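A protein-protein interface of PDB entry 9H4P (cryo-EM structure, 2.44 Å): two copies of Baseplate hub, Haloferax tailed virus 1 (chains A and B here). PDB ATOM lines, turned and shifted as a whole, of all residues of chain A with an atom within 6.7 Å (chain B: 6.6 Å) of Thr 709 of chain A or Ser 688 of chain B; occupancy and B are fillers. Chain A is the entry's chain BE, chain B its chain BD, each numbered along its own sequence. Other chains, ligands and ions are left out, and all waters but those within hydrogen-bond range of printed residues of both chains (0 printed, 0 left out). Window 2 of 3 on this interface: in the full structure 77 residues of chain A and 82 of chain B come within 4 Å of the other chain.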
ATOM      1  N   VAL A 690     -22.392   2.593 -23.596  1.00  0.00           N
ATOM      2  CA  VAL A 690     -21.556   1.383 -23.485  1.00  0.00           C
ATOM      3  C   VAL A 690     -20.157   1.754 -22.984  1.00  0.00           C
ATOM      4  O   VAL A 690     -19.233   1.900 -23.787  1.00  0.00           O
ATOM      5  CB  VAL A 690     -21.513   0.634 -24.831  1.00  0.00           C
ATOM      6  CG1 VAL A 690     -20.777  -0.703 -24.715  1.00  0.00           C
ATOM      7  CG2 VAL A 690     -22.906   0.335 -25.395  1.00  0.00           C
ATOM      8  N   PRO A 691     -19.978   1.971 -21.672  1.00  0.00           N
ATOM      9  CA  PRO A 691     -18.785   2.622 -21.140  1.00  0.00           C
ATOM     10  C   PRO A 691     -17.548   1.729 -21.016  1.00  0.00           C
ATOM     11  O   PRO A 691     -16.456   2.261 -20.818  1.00  0.00           O
ATOM     12  CB  PRO A 691     -19.202   3.126 -19.761  1.00  0.00           C
ATOM     13  CG  PRO A 691     -20.253   2.113 -19.324  1.00  0.00           C
ATOM     14  CD  PRO A 691     -20.981   1.826 -20.630  1.00  0.00           C
ATOM     15  N   ILE A 692     -17.676   0.405 -21.103  1.00  0.00           N
ATOM     16  CA  ILE A 692     -16.578  -0.534 -20.834  1.00  0.00           C
ATOM     17  C   ILE A 692     -16.508  -1.583 -21.948  1.00  0.00           C
ATOM     18  O   ILE A 692     -17.505  -2.243 -22.236  1.00  0.00           O
ATOM     19  CB  ILE A 692     -16.764  -1.171 -19.442  1.00  0.00           C
ATOM     20  CG1 ILE A 692     -16.736  -0.119 -18.312  1.00  0.00           C
ATOM     21  CG2 ILE A 692     -15.693  -2.225 -19.176  1.00  0.00           C
ATOM     22  CD1 ILE A 692     -17.169  -0.663 -16.950  1.00  0.00           C
ATOM     23  N   GLY A 693     -15.332  -1.750 -22.557  1.00  0.00           N
ATOM     24  CA  GLY A 693     -15.085  -2.688 -23.659  1.00  0.00           C
ATOM     25  C   GLY A 693     -14.465  -4.026 -23.241  1.00  0.00           C
ATOM     26  O   GLY A 693     -13.866  -4.155 -22.171  1.00  0.00           O
ATOM     27  N   ASP A 704     -15.958   6.297 -12.365  1.00  0.00           N
ATOM     28  CA  ASP A 704     -17.169   6.803 -13.014  1.00  0.00           C
ATOM     29  C   ASP A 704     -17.403   6.084 -14.346  1.00  0.00           C
ATOM     30  O   ASP A 704     -16.466   5.912 -15.122  1.00  0.00           O
ATOM     31  CB  ASP A 704     -17.045   8.307 -13.245  1.00  0.00           C
ATOM     32  CG  ASP A 704     -18.152   8.830 -14.163  1.00  0.00           C
ATOM     33  OD1 ASP A 704     -19.339   8.521 -13.923  1.00  0.00           O
ATOM     34  OD2 ASP A 704     -17.793   9.496 -15.156  1.00  0.00           O
ATOM     35  N   LEU A 705     -18.639   5.696 -14.625  1.00  0.00           N
ATOM     36  CA  LEU A 705     -19.047   5.151 -15.914  1.00  0.00           C
ATOM     37  C   LEU A 705     -19.680   6.209 -16.829  1.00  0.00           C
ATOM     38  O   LEU A 705     -19.612   6.057 -18.044  1.00  0.00           O
ATOM     39  CB  LEU A 705     -20.012   3.978 -15.670  1.00  0.00           C
ATOM     40  CG  LEU A 705     -19.305   2.624 -15.478  1.00  0.00           C
ATOM     41  CD1 LEU A 705     -18.342   2.587 -14.298  1.00  0.00           C
ATOM     42  CD2 LEU A 705     -20.341   1.527 -15.258  1.00  0.00           C
ATOM     43  N   ALA A 706     -20.316   7.258 -16.308  1.00  0.00           N
ATOM     44  CA  ALA A 706     -21.132   8.148 -17.133  1.00  0.00           C
ATOM     45  C   ALA A 706     -20.302   9.061 -18.048  1.00  0.00           C
ATOM     46  O   ALA A 706     -20.560   9.126 -19.246  1.00  0.00           O
ATOM     47  CB  ALA A 706     -22.047   8.961 -16.226  1.00  0.00           C
ATOM     48  N   ASN A 707     -19.289   9.728 -17.498  1.00  0.00           N
ATOM     49  CA  ASN A 707     -18.472  10.740 -18.167  1.00  0.00           C
ATOM     50  C   ASN A 707     -17.005  10.299 -18.352  1.00  0.00           C
ATOM     51  O   ASN A 707     -16.137  11.100 -18.679  1.00  0.00           O
ATOM     52  CB  ASN A 707     -18.651  12.079 -17.424  1.00  0.00           C
ATOM     53  CG  ASN A 707     -19.810  12.892 -17.993  1.00  0.00           C
ATOM     54  OD1 ASN A 707     -20.956  12.475 -17.970  1.00  0.00           O
ATOM     55  ND2 ASN A 707     -19.545  14.049 -18.553  1.00  0.00           N
ATOM     56  N   ASN A 708     -16.713   9.008 -18.207  1.00  0.00           N
ATOM     57  CA  ASN A 708     -15.411   8.393 -18.474  1.00  0.00           C
ATOM     58  C   ASN A 708     -15.626   7.045 -19.174  1.00  0.00           C
ATOM     59  O   ASN A 708     -16.680   6.434 -19.015  1.00  0.00           O
ATOM     60  CB  ASN A 708     -14.649   8.215 -17.152  1.00  0.00           C
ATOM     61  CG  ASN A 708     -14.238   9.525 -16.516  1.00  0.00           C
ATOM     62  OD1 ASN A 708     -13.131   9.995 -16.712  1.00  0.00           O
ATOM     63  ND2 ASN A 708     -15.075  10.138 -15.715  1.00  0.00           N
ATOM     64  N   THR A 709     -14.662   6.549 -19.953  1.00  0.00           N
ATOM     65  CA  THR A 709     -14.817   5.241 -20.618  1.00  0.00           C
ATOM     66  C   THR A 709     -13.506   4.517 -20.914  1.00  0.00           C
ATOM     67  O   THR A 709     -12.472   5.127 -21.168  1.00  0.00           O
ATOM     68  CB  THR A 709     -15.682   5.371 -21.873  1.00  0.00           C
ATOM     69  OG1 THR A 709     -15.840   4.144 -22.529  1.00  0.00           O
ATOM     70  CG2 THR A 709     -15.094   6.307 -22.913  1.00  0.00           C
ATOM     71  N   PHE A 710     -13.586   3.185 -20.915  1.00  0.00           N
ATOM     72  CA  PHE A 710     -12.454   2.269 -20.980  1.00  0.00           C
ATOM     73  C   PHE A 710     -12.667   1.291 -22.142  1.00  0.00           C
ATOM     74  O   PHE A 710     -13.356   0.282 -22.000  1.00  0.00           O
ATOM     75  CB  PHE A 710     -12.332   1.563 -19.618  1.00  0.00           C
ATOM     76  CG  PHE A 710     -12.361   2.497 -18.421  1.00  0.00           C
ATOM     77  CD1 PHE A 710     -11.194   3.145 -17.990  1.00  0.00           C
ATOM     78  CD2 PHE A 710     -13.581   2.756 -17.771  1.00  0.00           C
ATOM     79  CE1 PHE A 710     -11.250   4.048 -16.915  1.00  0.00           C
ATOM     80  CE2 PHE A 710     -13.637   3.663 -16.703  1.00  0.00           C
ATOM     81  CZ  PHE A 710     -12.470   4.310 -16.275  1.00  0.00           C
ATOM     82  N   GLY A 711     -12.180   1.625 -23.334  1.00  0.00           N
ATOM     83  CA  GLY A 711     -12.407   0.833 -24.550  1.00  0.00           C
ATOM     84  C   GLY A 711     -13.865   0.799 -25.039  1.00  0.00           C
ATOM     85  O   GLY A 711     -14.174   0.071 -25.982  1.00  0.00           O
ATOM     86  N   GLY A 712     -14.767   1.541 -24.399  1.00  0.00           N
ATOM     87  CA  GLY A 712     -16.204   1.505 -24.664  1.00  0.00           C
ATOM     88  C   GLY A 712     -16.607   2.134 -25.998  1.00  0.00           C
ATOM     89  O   GLY A 712     -15.856   2.898 -26.599  1.00  0.00           O
ATOM     90  N   SER A 713     -17.825   1.839 -26.449  1.00  0.00           N
ATOM     91  CA  SER A 713     -18.370   2.345 -27.715  1.00  0.00           C
ATOM     92  C   SER A 713     -19.024   3.732 -27.608  1.00  0.00           C
ATOM     93  O   SER A 713     -19.009   4.499 -28.566  1.00  0.00           O
ATOM     94  CB  SER A 713     -19.362   1.316 -28.265  1.00  0.00           C
ATOM     95  OG  SER A 713     -19.845   1.696 -29.534  1.00  0.00           O
ATOM     96  N   SER A 714     -19.606   4.082 -26.454  1.00  0.00           N
ATOM     97  CA  SER A 714     -20.319   5.353 -26.248  1.00  0.00           C
ATOM     98  C   SER A 714     -20.465   5.690 -24.758  1.00  0.00           C
ATOM     99  O   SER A 714     -20.480   4.785 -23.930  1.00  0.00           O
ATOM    100  CB  SER A 714     -21.689   5.262 -26.922  1.00  0.00           C
ATOM    101  OG  SER A 714     -22.420   6.451 -26.749  1.00  0.00           O
ATOM    102  N   THR A 715     -20.622   6.966 -24.397  1.00  0.00           N
ATOM    103  CA  THR A 715     -20.799   7.433 -23.005  1.00  0.00           C
ATOM    104  C   THR A 715     -22.148   8.113 -22.791  1.00  0.00           C
ATOM    105  O   THR A 715     -22.917   8.278 -23.734  1.00  0.00           O
ATOM    106  CB  THR A 715     -19.662   8.370 -22.582  1.00  0.00           C
ATOM    107  OG1 THR A 715     -19.673   9.555 -23.335  1.00  0.00           O
ATOM    108  CG2 THR A 715     -18.315   7.685 -22.760  1.00  0.00           C
ATOM    109  N   THR B 677      -2.417   2.618 -27.894  1.00  0.00           N
ATOM    110  CA  THR B 677      -3.600   3.106 -27.176  1.00  0.00           C
ATOM    111  C   THR B 677      -3.669   4.630 -27.233  1.00  0.00           C
ATOM    112  O   THR B 677      -2.659   5.305 -27.031  1.00  0.00           O
ATOM    113  CB  THR B 677      -3.567   2.636 -25.719  1.00  0.00           C
ATOM    114  OG1 THR B 677      -3.617   1.230 -25.694  1.00  0.00           O
ATOM    115  CG2 THR B 677      -4.740   3.128 -24.876  1.00  0.00           C
ATOM    116  N   VAL B 678      -4.853   5.179 -27.493  1.00  0.00           N
ATOM    117  CA  VAL B 678      -5.132   6.617 -27.442  1.00  0.00           C
ATOM    118  C   VAL B 678      -6.001   6.914 -26.228  1.00  0.00           C
ATOM    119  O   VAL B 678      -7.037   6.280 -26.037  1.00  0.00           O
ATOM    120  CB  VAL B 678      -5.826   7.098 -28.726  1.00  0.00           C
ATOM    121  CG1 VAL B 678      -6.062   8.611 -28.680  1.00  0.00           C
ATOM    122  CG2 VAL B 678      -4.985   6.794 -29.966  1.00  0.00           C
ATOM    123  N   THR B 679      -5.598   7.887 -25.417  1.00  0.00           N
ATOM    124  CA  THR B 679      -6.426   8.451 -24.346  1.00  0.00           C
ATOM    125  C   THR B 679      -6.676   9.925 -24.625  1.00  0.00           C
ATOM    126  O   THR B 679      -5.729  10.699 -24.729  1.00  0.00           O
ATOM    127  CB  THR B 679      -5.768   8.244 -22.976  1.00  0.00           C
ATOM    128  OG1 THR B 679      -5.771   6.876 -22.643  1.00  0.00           O
ATOM    129  CG2 THR B 679      -6.483   8.974 -21.839  1.00  0.00           C
ATOM    130  N   LEU B 680      -7.941  10.320 -24.705  1.00  0.00           N
ATOM    131  CA  LEU B 680      -8.382  11.705 -24.829  1.00  0.00           C
ATOM    132  C   LEU B 680      -9.000  12.165 -23.504  1.00  0.00           C
ATOM    133  O   LEU B 680      -9.888  11.518 -22.958  1.00  0.00           O
ATOM    134  CB  LEU B 680      -9.331  11.802 -26.031  1.00  0.00           C
ATOM    135  CG  LEU B 680      -9.740  13.236 -26.398  1.00  0.00           C
ATOM    136  CD1 LEU B 680      -9.954  13.354 -27.903  1.00  0.00           C
ATOM    137  CD2 LEU B 680     -11.043  13.636 -25.726  1.00  0.00           C
ATOM    138  N   ASP B 685     -12.339  14.389 -17.687  1.00  0.00           N
ATOM    139  CA  ASP B 685     -13.118  13.288 -18.270  1.00  0.00           C
ATOM    140  C   ASP B 685     -12.264  12.520 -19.285  1.00  0.00           C
ATOM    141  O   ASP B 685     -11.937  13.055 -20.346  1.00  0.00           O
ATOM    142  CB  ASP B 685     -14.393  13.814 -18.951  1.00  0.00           C
ATOM    143  CG  ASP B 685     -15.490  14.325 -18.007  1.00  0.00           C
ATOM    144  OD1 ASP B 685     -15.290  14.351 -16.773  1.00  0.00           O
ATOM    145  OD2 ASP B 685     -16.565  14.721 -18.521  1.00  0.00           O
ATOM    146  N   THR B 686     -11.888  11.267 -18.998  1.00  0.00           N
ATOM    147  CA  THR B 686     -10.983  10.482 -19.849  1.00  0.00           C
ATOM    148  C   THR B 686     -11.703   9.399 -20.645  1.00  0.00           C
ATOM    149  O   THR B 686     -12.368   8.522 -20.087  1.00  0.00           O
ATOM    150  CB  THR B 686      -9.835   9.835 -19.068  1.00  0.00           C
ATOM    151  OG1 THR B 686     -10.314   8.948 -18.088  1.00  0.00           O
ATOM    152  CG2 THR B 686      -8.943  10.859 -18.385  1.00  0.00           C
ATOM    153  N   TYR B 687     -11.474   9.422 -21.952  1.00  0.00           N
ATOM    154  CA  TYR B 687     -12.001   8.515 -22.961  1.00  0.00           C
ATOM    155  C   TYR B 687     -10.818   7.776 -23.598  1.00  0.00           C
ATOM    156  O   TYR B 687      -9.930   8.425 -24.140  1.00  0.00           O
ATOM    157  CB  TYR B 687     -12.773   9.355 -23.993  1.00  0.00           C
ATOM    158  CG  TYR B 687     -13.868  10.239 -23.409  1.00  0.00           C
ATOM    159  CD1 TYR B 687     -13.541  11.485 -22.843  1.00  0.00           C
ATOM    160  CD2 TYR B 687     -15.213   9.822 -23.420  1.00  0.00           C
ATOM    161  CE1 TYR B 687     -14.533  12.276 -22.237  1.00  0.00           C
ATOM    162  CE2 TYR B 687     -16.205  10.609 -22.810  1.00  0.00           C
ATOM    163  CZ  TYR B 687     -15.866  11.827 -22.196  1.00  0.00           C
ATOM    164  OH  TYR B 687     -16.830  12.562 -21.589  1.00  0.00           O
ATOM    165  N   SER B 688     -10.764   6.441 -23.546  1.00  0.00           N
ATOM    166  CA  SER B 688      -9.608   5.677 -24.062  1.00  0.00           C
ATOM    167  C   SER B 688     -10.005   4.562 -25.022  1.00  0.00           C
ATOM    168  O   SER B 688     -10.985   3.860 -24.774  1.00  0.00           O
ATOM    169  CB  SER B 688      -8.775   5.079 -22.929  1.00  0.00           C
ATOM    170  OG  SER B 688      -8.344   6.087 -22.037  1.00  0.00           O
ATOM    171  N   TRP B 689      -9.228   4.358 -26.088  1.00  0.00           N
ATOM    172  CA  TRP B 689      -9.473   3.327 -27.101  1.00  0.00           C
ATOM    173  C   TRP B 689      -8.181   2.822 -27.755  1.00  0.00           C
ATOM    174  O   TRP B 689      -7.130   3.453 -27.658  1.00  0.00           O
ATOM    175  CB  TRP B 689     -10.465   3.841 -28.149  1.00  0.00           C
ATOM    176  CG  TRP B 689      -9.972   4.884 -29.104  1.00  0.00           C
ATOM    177  CD1 TRP B 689      -9.583   4.657 -30.377  1.00  0.00           C
ATOM    178  CD2 TRP B 689      -9.830   6.323 -28.898  1.00  0.00           C
ATOM    179  NE1 TRP B 689      -9.220   5.843 -30.975  1.00  0.00           N
ATOM    180  CE2 TRP B 689      -9.365   6.905 -30.114  1.00  0.00           C
ATOM    181  CE3 TRP B 689     -10.055   7.198 -27.818  1.00  0.00           C
ATOM    182  CZ2 TRP B 689      -9.144   8.280 -30.256  1.00  0.00           C
ATOM    183  CZ3 TRP B 689      -9.807   8.575 -27.938  1.00  0.00           C
ATOM    184  CH2 TRP B 689      -9.364   9.122 -29.156  1.00  0.00           C
ATOM    185  N   VAL B 690      -8.247   1.660 -28.406  1.00  0.00           N
ATOM    186  CA  VAL B 690      -7.083   0.966 -28.975  1.00  0.00           C
ATOM    187  C   VAL B 690      -7.258   0.805 -30.488  1.00  0.00           C
ATOM    188  O   VAL B 690      -7.821  -0.198 -30.932  1.00  0.00           O
ATOM    189  CB  VAL B 690      -6.852  -0.385 -28.267  1.00  0.00           C
ATOM    190  CG1 VAL B 690      -5.552  -1.033 -28.742  1.00  0.00           C
ATOM    191  CG2 VAL B 690      -6.781  -0.223 -26.747  1.00  0.00           C
ATOM    192  N   SER B 714     -11.219  -1.148 -30.611  1.00  0.00           N
ATOM    193  CA  SER B 714     -12.277  -0.147 -30.405  1.00  0.00           C
ATOM    194  C   SER B 714     -11.914   1.251 -30.930  1.00  0.00           C
ATOM    195  O   SER B 714     -10.734   1.586 -31.015  1.00  0.00           O
ATOM    196  CB  SER B 714     -12.622  -0.102 -28.915  1.00  0.00           C
ATOM    197  OG  SER B 714     -13.820   0.607 -28.696  1.00  0.00           O
ATOM    198  N   THR B 715     -12.917   2.060 -31.278  1.00  0.00           N
ATOM    199  CA  THR B 715     -12.806   3.431 -31.828  1.00  0.00           C
ATOM    200  C   THR B 715     -12.909   4.516 -30.751  1.00  0.00           C
ATOM    201  O   THR B 715     -13.215   4.235 -29.593  1.00  0.00           O
ATOM    202  CB  THR B 715     -13.931   3.680 -32.852  1.00  0.00           C
ATOM    203  OG1 THR B 715     -15.202   3.516 -32.264  1.00  0.00           O
ATOM    204  CG2 THR B 715     -13.828   2.758 -34.059  1.00  0.00           C
ATOM    205  N   PRO B 717     -15.200   7.038 -28.766  1.00  0.00           N
ATOM    206  CA  PRO B 717     -16.571   6.804 -28.300  1.00  0.00           C
ATOM    207  C   PRO B 717     -17.587   7.897 -28.692  1.00  0.00           C
ATOM    208  O   PRO B 717     -18.597   8.072 -28.016  1.00  0.00           O
ATOM    209  CB  PRO B 717     -16.436   6.640 -26.784  1.00  0.00           C
ATOM    210  CG  PRO B 717     -15.287   7.586 -26.464  1.00  0.00           C
ATOM    211  CD  PRO B 717     -14.352   7.377 -27.640  1.00  0.00           C
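3 positions are printed for both chains.
Of the 15 pairs that touch across the chains among the printed residues, none has its exchanged pair printed and touching as well.
Of the printed residues of chain B, Asn 707 of chain A touches Asp 685 and Tyr 687.
Printed residues of chain B within 4 Å of Asn 708 of chain A: Asp 685 and Thr 686.
Thr 709 of chain A touches just these residues of chain B: Thr 686, Tyr 687, Ser 688 and Pro 717.
Printed residues of chain B within 4 Å of Ser 714 of chain A: Pro 717.
Thr 677 of chain B touches none of the printed residues of chain A.
Thr 679 of chain B touches none of the printed residues of chain A.
Printed residues of chain A within 4 Å of Thr 686 of chain B: Asn 708 (2.9 Å) and Thr 709 (3.0 Å).
Of the printed residues of chain A, Tyr 687 of chain B touches Asn 707 (3.3 Å), Thr 709 (3.6 Å) and Thr 715 (3.6 Å).
Ser 688 of chain B touches just these residues of chain A: Thr 709 and Gly 711.
The nearest residue of chain B that does not touch Thr 709 of chain A is Trp 689 of chain B (5.9 Å).
Among the printed residues, 15 pairs touch across the chains.
Among the printed residues, no Asp or Glu carboxylate lies within 4 Å of a Lys or Arg side-chain nitrogen of the other chain.
The side-chain amide nitrogen (ND2) of Asn 707 of chain A sits at hydrogen-bond distance from the side-chain carboxylate (OD2) of Asp 685 of chain B, at 3.1 Å.
The backbone NH of Thr 686 of chain B lies within hydrogen-bond range of the side-chain amide oxygen of Asn 708 of chain A.
The backbone carbonyl oxygen (O) of Thr 686 of chain B sits at hydrogen-bond distance from the backbone NH (N) of Thr 709 of chain A, 3.0 Å away.
The side-chain hydroxyl (OH) of Tyr 687 of chain B sits at hydrogen-bond distance from the backbone carbonyl oxygen (O) of Asn 707 of chain A, at 3.3 Å.
O of Thr 709 of chain A lies within hydrogen-bond range of N of Ser 688 of chain B (3.2 Å).
The backbone NH (N) of Gly 711 of chain A lies within hydrogen-bond range of the backbone carbonyl oxygen (O) of Ser 688 of chain B, at 2.9 Å.
The side-chain hydroxyl (OG) of Ser 714 of chain B lies within hydrogen-bond range of the backbone carbonyl oxygen (O) of Gly 711 of chain A (2.8 Å).
OG1 of Thr 679 of chain B is in hydrogen-bond range of OG of Ser 688 of chain B, 2.8 Å away.
N of Ser 713 of chain A sits at hydrogen-bond distance from O of Val 690 of chain A (3.0 Å).
O of Pro 691 of chain A is in hydrogen-bond range of OG1 of Thr 709 of chain A (2.6 Å).
The side-chain carboxylate of Asp 704 of chain A is in hydrogen-bond range of the backbone NH of Asn 707 of chain A, at 2.8 Å.
The side-chain carboxylate (OD2) of Asp 704 of chain A is in hydrogen-bond range of the side-chain amide nitrogen (ND2) of Asn 708 of chain A, at 2.8 Å.
The side-chain hydroxyl (OG1) of Thr 709 of chain A lies within hydrogen-bond range of the backbone NH (N) of Gly 712 of chain A (3.4 Å).
Among the printed residues, pairs that only touch across the chains: Ser 713 of chain A with Pro 717 of chain B (3.4 Å), Thr 709 of chain A with Tyr 687 of chain B (3.6 Å), Thr 715 of chain A with Tyr 687 of chain B (3.6 Å), Asn 708 of chain A with Asp 685 of chain B (3.6 Å), Ser 714 of chain A with Pro 717 of chain B (3.7 Å), Gly 712 of chain A with Ser 714 of chain B (3.7 Å), Thr 709 of chain A with Pro 717 of chain B (3.8 Å) and Gly 712 of chain A with Pro 717 of chain B (3.8 Å).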
